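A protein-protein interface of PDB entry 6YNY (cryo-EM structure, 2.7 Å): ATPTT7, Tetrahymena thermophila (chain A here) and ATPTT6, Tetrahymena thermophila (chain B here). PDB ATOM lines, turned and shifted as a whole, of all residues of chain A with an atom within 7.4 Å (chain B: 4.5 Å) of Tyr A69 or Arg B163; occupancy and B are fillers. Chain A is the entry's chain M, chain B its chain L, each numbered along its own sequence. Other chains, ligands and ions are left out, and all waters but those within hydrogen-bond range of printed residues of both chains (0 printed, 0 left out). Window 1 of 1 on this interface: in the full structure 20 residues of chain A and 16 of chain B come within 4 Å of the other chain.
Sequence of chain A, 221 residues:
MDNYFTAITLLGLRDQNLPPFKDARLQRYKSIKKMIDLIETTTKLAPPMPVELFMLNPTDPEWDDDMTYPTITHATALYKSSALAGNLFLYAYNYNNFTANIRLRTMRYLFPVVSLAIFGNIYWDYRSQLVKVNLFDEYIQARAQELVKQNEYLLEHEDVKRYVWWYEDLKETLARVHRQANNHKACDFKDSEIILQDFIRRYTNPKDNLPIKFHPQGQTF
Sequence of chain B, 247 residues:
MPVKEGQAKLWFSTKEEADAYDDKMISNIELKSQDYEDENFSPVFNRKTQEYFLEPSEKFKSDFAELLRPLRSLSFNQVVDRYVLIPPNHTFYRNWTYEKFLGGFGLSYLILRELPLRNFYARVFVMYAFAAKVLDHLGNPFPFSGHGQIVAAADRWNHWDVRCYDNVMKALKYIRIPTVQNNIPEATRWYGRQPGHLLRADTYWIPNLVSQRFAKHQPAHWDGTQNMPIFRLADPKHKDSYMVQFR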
ATOM      1  N   ASP A  66     -24.623  -0.787  31.047  1.00  0.00           N
ATOM      2  CA  ASP A  66     -25.092   0.462  30.459  1.00  0.00           C
ATOM      3  C   ASP A  66     -24.006   1.528  30.535  1.00  0.00           C
ATOM      4  O   ASP A  66     -24.241   2.674  30.921  1.00  0.00           O
ATOM      5  CB  ASP A  66     -26.378   0.931  31.135  1.00  0.00           C
ATOM      6  CG  ASP A  66     -27.576   0.086  30.757  1.00  0.00           C
ATOM      7  OD1 ASP A  66     -27.433  -0.787  29.877  1.00  0.00           O
ATOM      8  OD2 ASP A  66     -28.660   0.294  31.338  1.00  0.00           O
ATOM      9  N   MET A  67     -22.797   1.130  30.165  1.00  0.00           N
ATOM     10  CA  MET A  67     -21.649   2.008  30.282  1.00  0.00           C
ATOM     11  C   MET A  67     -21.700   3.124  29.246  1.00  0.00           C
ATOM     12  O   MET A  67     -22.251   2.968  28.154  1.00  0.00           O
ATOM     13  CB  MET A  67     -20.360   1.209  30.123  1.00  0.00           C
ATOM     14  CG  MET A  67     -19.116   2.005  30.374  1.00  0.00           C
ATOM     15  SD  MET A  67     -19.101   2.739  32.010  1.00  0.00           S
ATOM     16  CE  MET A  67     -17.618   3.706  31.883  1.00  0.00           C
ATOM     17  N   THR A  68     -21.115   4.258  29.606  1.00  0.00           N
ATOM     18  CA  THR A  68     -21.055   5.426  28.746  1.00  0.00           C
ATOM     19  C   THR A  68     -19.699   5.513  28.059  1.00  0.00           C
ATOM     20  O   THR A  68     -18.754   4.793  28.386  1.00  0.00           O
ATOM     21  CB  THR A  68     -21.313   6.700  29.553  1.00  0.00           C
ATOM     22  OG1 THR A  68     -20.323   6.832  30.576  1.00  0.00           O
ATOM     23  CG2 THR A  68     -22.668   6.655  30.186  1.00  0.00           C
ATOM     24  N   TYR A  69     -19.614   6.423  27.094  1.00  0.00           N
ATOM     25  CA  TYR A  69     -18.369   6.679  26.389  1.00  0.00           C
ATOM     26  C   TYR A  69     -17.611   7.785  27.109  1.00  0.00           C
ATOM     27  O   TYR A  69     -18.079   8.932  27.119  1.00  0.00           O
ATOM     28  CB  TYR A  69     -18.635   7.082  24.949  1.00  0.00           C
ATOM     29  CG  TYR A  69     -18.947   5.939  24.019  1.00  0.00           C
ATOM     30  CD1 TYR A  69     -17.934   5.168  23.481  1.00  0.00           C
ATOM     31  CD2 TYR A  69     -20.250   5.644  23.659  1.00  0.00           C
ATOM     32  CE1 TYR A  69     -18.207   4.134  22.627  1.00  0.00           C
ATOM     33  CE2 TYR A  69     -20.531   4.609  22.804  1.00  0.00           C
ATOM     34  CZ  TYR A  69     -19.507   3.856  22.291  1.00  0.00           C
ATOM     35  OH  TYR A  69     -19.783   2.822  21.434  1.00  0.00           O
ATOM     36  N   PRO A  70     -16.464   7.503  27.725  1.00  0.00           N
ATOM     37  CA  PRO A  70     -15.665   8.586  28.308  1.00  0.00           C
ATOM     38  C   PRO A  70     -14.983   9.399  27.219  1.00  0.00           C
ATOM     39  O   PRO A  70     -14.389   8.848  26.292  1.00  0.00           O
ATOM     40  CB  PRO A  70     -14.653   7.843  29.184  1.00  0.00           C
ATOM     41  CG  PRO A  70     -14.532   6.528  28.567  1.00  0.00           C
ATOM     42  CD  PRO A  70     -15.866   6.189  27.998  1.00  0.00           C
ATOM     43  N   THR A  71     -15.081  10.720  27.333  1.00  0.00           N
ATOM     44  CA  THR A  71     -14.540  11.628  26.339  1.00  0.00           C
ATOM     45  C   THR A  71     -13.607  12.623  27.008  1.00  0.00           C
ATOM     46  O   THR A  71     -13.516  12.705  28.234  1.00  0.00           O
ATOM     47  CB  THR A  71     -15.644  12.396  25.599  1.00  0.00           C
ATOM     48  OG1 THR A  71     -16.110  13.473  26.417  1.00  0.00           O
ATOM     49  CG2 THR A  71     -16.804  11.495  25.288  1.00  0.00           C
ATOM     50  N   ILE A  72     -12.906  13.378  26.171  1.00  0.00           N
ATOM     51  CA  ILE A  72     -12.088  14.501  26.601  1.00  0.00           C
ATOM     52  C   ILE A  72     -12.718  15.769  26.052  1.00  0.00           C
ATOM     53  O   ILE A  72     -12.957  15.880  24.844  1.00  0.00           O
ATOM     54  CB  ILE A  72     -10.633  14.356  26.129  1.00  0.00           C
ATOM     55  CG1 ILE A  72      -9.972  13.171  26.821  1.00  0.00           C
ATOM     56  CG2 ILE A  72      -9.869  15.625  26.408  1.00  0.00           C
ATOM     57  CD1 ILE A  72      -8.673  12.769  26.214  1.00  0.00           C
ATOM     58  N   VAL A 133     -10.250   7.416  29.418  1.00  0.00           N
ATOM     59  CA  VAL A 133     -10.356   7.040  28.015  1.00  0.00           C
ATOM     60  C   VAL A 133      -9.429   5.875  27.703  1.00  0.00           C
ATOM     61  O   VAL A 133      -9.788   4.962  26.951  1.00  0.00           O
ATOM     62  CB  VAL A 133     -10.055   8.255  27.124  1.00  0.00           C
ATOM     63  CG1 VAL A 133      -9.931   7.838  25.686  1.00  0.00           C
ATOM     64  CG2 VAL A 133     -11.137   9.295  27.274  1.00  0.00           C
ATOM     65  N   PHE A 136     -10.677   2.605  29.074  1.00  0.00           N
ATOM     66  CA  PHE A 136     -11.783   2.102  28.273  1.00  0.00           C
ATOM     67  C   PHE A 136     -11.282   1.462  26.989  1.00  0.00           C
ATOM     68  O   PHE A 136     -11.758   0.392  26.594  1.00  0.00           O
ATOM     69  CB  PHE A 136     -12.743   3.247  27.973  1.00  0.00           C
ATOM     70  CG  PHE A 136     -13.921   2.858  27.142  1.00  0.00           C
ATOM     71  CD1 PHE A 136     -15.055   2.343  27.731  1.00  0.00           C
ATOM     72  CD2 PHE A 136     -13.902   3.026  25.774  1.00  0.00           C
ATOM     73  CE1 PHE A 136     -16.139   1.994  26.967  1.00  0.00           C
ATOM     74  CE2 PHE A 136     -14.981   2.679  25.013  1.00  0.00           C
ATOM     75  CZ  PHE A 136     -16.103   2.163  25.608  1.00  0.00           C
ATOM     76  N   ASP A 137     -10.316   2.098  26.327  1.00  0.00           N
ATOM     77  CA  ASP A 137      -9.808   1.564  25.072  1.00  0.00           C
ATOM     78  C   ASP A 137      -9.104   0.230  25.281  1.00  0.00           C
ATOM     79  O   ASP A 137      -9.246  -0.686  24.464  1.00  0.00           O
ATOM     80  CB  ASP A 137      -8.863   2.571  24.420  1.00  0.00           C
ATOM     81  CG  ASP A 137      -9.559   3.863  24.033  1.00  0.00           C
ATOM     82  OD1 ASP A 137     -10.804   3.868  23.945  1.00  0.00           O
ATOM     83  OD2 ASP A 137      -8.860   4.872  23.805  1.00  0.00           O
ATOM     84  N   ILE A 140     -11.894  -2.799  26.073  1.00  0.00           N
ATOM     85  CA  ILE A 140     -12.694  -3.297  24.961  1.00  0.00           C
ATOM     86  C   ILE A 140     -11.855  -4.167  24.040  1.00  0.00           C
ATOM     87  O   ILE A 140     -12.376  -5.083  23.393  1.00  0.00           O
ATOM     88  CB  ILE A 140     -13.325  -2.118  24.202  1.00  0.00           C
ATOM     89  CG1 ILE A 140     -12.238  -1.205  23.646  1.00  0.00           C
ATOM     90  CG2 ILE A 140     -14.239  -1.338  25.121  1.00  0.00           C
ATOM     91  CD1 ILE A 140     -12.759  -0.134  22.758  1.00  0.00           C
ATOM     92  N   ARG B 156     -17.021   6.838  10.434  1.00  0.00           N
ATOM     93  CA  ARG B 156     -17.412   5.948  11.515  1.00  0.00           C
ATOM     94  C   ARG B 156     -17.382   6.626  12.875  1.00  0.00           C
ATOM     95  O   ARG B 156     -17.921   6.069  13.837  1.00  0.00           O
ATOM     96  CB  ARG B 156     -16.496   4.728  11.545  1.00  0.00           C
ATOM     97  CG  ARG B 156     -15.082   5.042  11.958  1.00  0.00           C
ATOM     98  CD  ARG B 156     -14.184   3.847  11.785  1.00  0.00           C
ATOM     99  NE  ARG B 156     -13.976   3.523  10.382  1.00  0.00           N
ATOM    100  CZ  ARG B 156     -13.329   2.448   9.955  1.00  0.00           C
ATOM    101  NH1 ARG B 156     -13.187   2.236   8.659  1.00  0.00           N
ATOM    102  NH2 ARG B 156     -12.830   1.581  10.823  1.00  0.00           N
ATOM    103  N   ASN B 158     -18.677   9.653  13.540  1.00  0.00           N
ATOM    104  CA  ASN B 158     -19.799  10.552  13.746  1.00  0.00           C
ATOM    105  C   ASN B 158     -20.596  10.107  14.963  1.00  0.00           C
ATOM    106  O   ASN B 158     -21.032   8.955  15.044  1.00  0.00           O
ATOM    107  CB  ASN B 158     -20.704  10.576  12.516  1.00  0.00           C
ATOM    108  CG  ASN B 158     -19.975  10.962  11.251  1.00  0.00           C
ATOM    109  OD1 ASN B 158     -20.172  10.353  10.203  1.00  0.00           O
ATOM    110  ND2 ASN B 158     -19.133  11.974  11.337  1.00  0.00           N
ATOM    111  N   HIS B 159     -20.786  11.018  15.913  1.00  0.00           N
ATOM    112  CA  HIS B 159     -21.578  10.740  17.107  1.00  0.00           C
ATOM    113  C   HIS B 159     -21.029   9.543  17.880  1.00  0.00           C
ATOM    114  O   HIS B 159     -21.785   8.746  18.436  1.00  0.00           O
ATOM    115  CB  HIS B 159     -23.044  10.501  16.745  1.00  0.00           C
ATOM    116  CG  HIS B 159     -23.768  11.718  16.269  1.00  0.00           C
ATOM    117  ND1 HIS B 159     -24.141  11.894  14.956  1.00  0.00           N
ATOM    118  CD2 HIS B 159     -24.213  12.808  16.935  1.00  0.00           C
ATOM    119  CE1 HIS B 159     -24.774  13.045  14.830  1.00  0.00           C
ATOM    120  NE2 HIS B 159     -24.831  13.620  16.016  1.00  0.00           N
ATOM    121  N   TRP B 160     -19.703   9.415  17.928  1.00  0.00           N
ATOM    122  CA  TRP B 160     -19.113   8.214  18.506  1.00  0.00           C
ATOM    123  C   TRP B 160     -19.322   8.135  20.012  1.00  0.00           C
ATOM    124  O   TRP B 160     -19.394   7.033  20.564  1.00  0.00           O
ATOM    125  CB  TRP B 160     -17.624   8.146  18.174  1.00  0.00           C
ATOM    126  CG  TRP B 160     -16.771   9.145  18.878  1.00  0.00           C
ATOM    127  CD1 TRP B 160     -16.324  10.326  18.378  1.00  0.00           C
ATOM    128  CD2 TRP B 160     -16.244   9.045  20.204  1.00  0.00           C
ATOM    129  NE1 TRP B 160     -15.557  10.972  19.308  1.00  0.00           N
ATOM    130  CE2 TRP B 160     -15.493  10.208  20.440  1.00  0.00           C
ATOM    131  CE3 TRP B 160     -16.338   8.089  21.217  1.00  0.00           C
ATOM    132  CZ2 TRP B 160     -14.843  10.441  21.643  1.00  0.00           C
ATOM    133  CZ3 TRP B 160     -15.694   8.324  22.406  1.00  0.00           C
ATOM    134  CH2 TRP B 160     -14.955   9.490  22.611  1.00  0.00           C
ATOM    135  N   ASP B 161     -19.421   9.273  20.689  1.00  0.00           N
ATOM    136  CA  ASP B 161     -19.556   9.303  22.137  1.00  0.00           C
ATOM    137  C   ASP B 161     -21.004   9.332  22.606  1.00  0.00           C
ATOM    138  O   ASP B 161     -21.248   9.502  23.803  1.00  0.00           O
ATOM    139  CB  ASP B 161     -18.800  10.503  22.707  1.00  0.00           C
ATOM    140  CG  ASP B 161     -19.157  11.797  22.020  1.00  0.00           C
ATOM    141  OD1 ASP B 161     -20.235  12.351  22.308  1.00  0.00           O
ATOM    142  OD2 ASP B 161     -18.354  12.264  21.186  1.00  0.00           O
ATOM    143  N   VAL B 162     -21.964   9.167  21.701  1.00  0.00           N
ATOM    144  CA  VAL B 162     -23.373   9.125  22.069  1.00  0.00           C
ATOM    145  C   VAL B 162     -24.059   7.919  21.444  1.00  0.00           C
ATOM    146  O   VAL B 162     -25.290   7.821  21.463  1.00  0.00           O
ATOM    147  CB  VAL B 162     -24.091  10.426  21.672  1.00  0.00           C
ATOM    148  CG1 VAL B 162     -23.671  11.552  22.577  1.00  0.00           C
ATOM    149  CG2 VAL B 162     -23.799  10.773  20.238  1.00  0.00           C
ATOM    150  N   ARG B 163     -23.280   6.992  20.888  1.00  0.00           N
ATOM    151  CA  ARG B 163     -23.882   5.795  20.317  1.00  0.00           C
ATOM    152  C   ARG B 163     -24.593   4.961  21.371  1.00  0.00           C
ATOM    153  O   ARG B 163     -25.479   4.174  21.027  1.00  0.00           O
ATOM    154  CB  ARG B 163     -22.823   4.942  19.619  1.00  0.00           C
ATOM    155  CG  ARG B 163     -22.054   5.643  18.526  1.00  0.00           C
ATOM    156  CD  ARG B 163     -22.970   6.191  17.461  1.00  0.00           C
ATOM    157  NE  ARG B 163     -22.238   6.734  16.324  1.00  0.00           N
ATOM    158  CZ  ARG B 163     -21.878   6.032  15.256  1.00  0.00           C
ATOM    159  NH1 ARG B 163     -21.215   6.620  14.277  1.00  0.00           N
ATOM    160  NH2 ARG B 163     -22.179   4.751  15.157  1.00  0.00           N
ATOM    161  N   CYS B 164     -24.235   5.123  22.643  1.00  0.00           N
ATOM    162  CA  CYS B 164     -24.851   4.331  23.695  1.00  0.00           C
ATOM    163  C   CYS B 164     -26.275   4.773  23.997  1.00  0.00           C
ATOM    164  O   CYS B 164     -27.056   3.975  24.520  1.00  0.00           O
ATOM    165  CB  CYS B 164     -23.997   4.391  24.960  1.00  0.00           C
ATOM    166  SG  CYS B 164     -23.375   6.022  25.393  1.00  0.00           S
ATOM    167  N   TYR B 165     -26.631   6.012  23.678  1.00  0.00           N
ATOM    168  CA  TYR B 165     -27.950   6.543  23.984  1.00  0.00           C
ATOM    169  C   TYR B 165     -28.927   6.221  22.861  1.00  0.00           C
ATOM    170  O   TYR B 165     -28.621   6.433  21.684  1.00  0.00           O
ATOM    171  CB  TYR B 165     -27.873   8.051  24.209  1.00  0.00           C
ATOM    172  CG  TYR B 165     -26.871   8.447  25.258  1.00  0.00           C
ATOM    173  CD1 TYR B 165     -27.139   8.270  26.602  1.00  0.00           C
ATOM    174  CD2 TYR B 165     -25.654   8.999  24.905  1.00  0.00           C
ATOM    175  CE1 TYR B 165     -26.227   8.626  27.561  1.00  0.00           C
ATOM    176  CE2 TYR B 165     -24.736   9.360  25.858  1.00  0.00           C
ATOM    177  CZ  TYR B 165     -25.027   9.170  27.186  1.00  0.00           C
ATOM    178  OH  TYR B 165     -24.116   9.528  28.144  1.00  0.00           O
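Of chain B, only Trp B160, Asp B161, Arg B163 and Cys B164 come within 4 Å of Tyr A69. Printed residues of chain B within 4 Å of Pro A70: Trp B160 (3.8 Å). Ile A72 touches none of the printed residues of chain B. Asp A137 touches none of the printed residues of chain B. Of the printed residues of chain A, Trp B160 touches Tyr A69 (3.5 Å), Pro A70 (3.8 Å) and Thr A71 (3.8 Å). Of the printed residues of chain A, Asp B161 touches Tyr A69 and Thr A71. Of the printed residues of chain A, Arg B163 touches Tyr A69 (3.9 Å). Of the printed residues of chain A, Cys B164 touches Met A67 and Tyr A69. The nearest printed residue of chain A that does not touch Arg B163 is Met A67 (7.4 Å).
The guanidinium group (NH1) of Arg B163 is in hydrogen-bond range of the backbone carbonyl oxygen (O) of Arg B156, at 3.4 Å. The guanidinium group of Arg B163 sits at hydrogen-bond distance from the backbone carbonyl oxygen of Asn B158 (2.5 Å). The backbone carbonyl oxygen (O) of His B159 sits at hydrogen-bond distance from the guanidinium group (NE) of Arg B163 (3.0 Å).
Hydrophobic or aromatic side chains of chain A that line the printed part of chain B: Tyr A69. Hydrophobic or aromatic side chains of chain B that line the printed part of chain A: Trp B160 and Tyr B165.
Among the printed residues, pairs that only touch across the chains: Thr A71 with Asp B161, Tyr A69 with Trp B160, Tyr A69 with Cys B164, Tyr A69 with Asp B161, Pro A70 with Trp B160, Thr A68 with Tyr B165, Thr A71 with Trp B160, Met A67 with Cys B164 and Tyr A69 with Arg B163.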
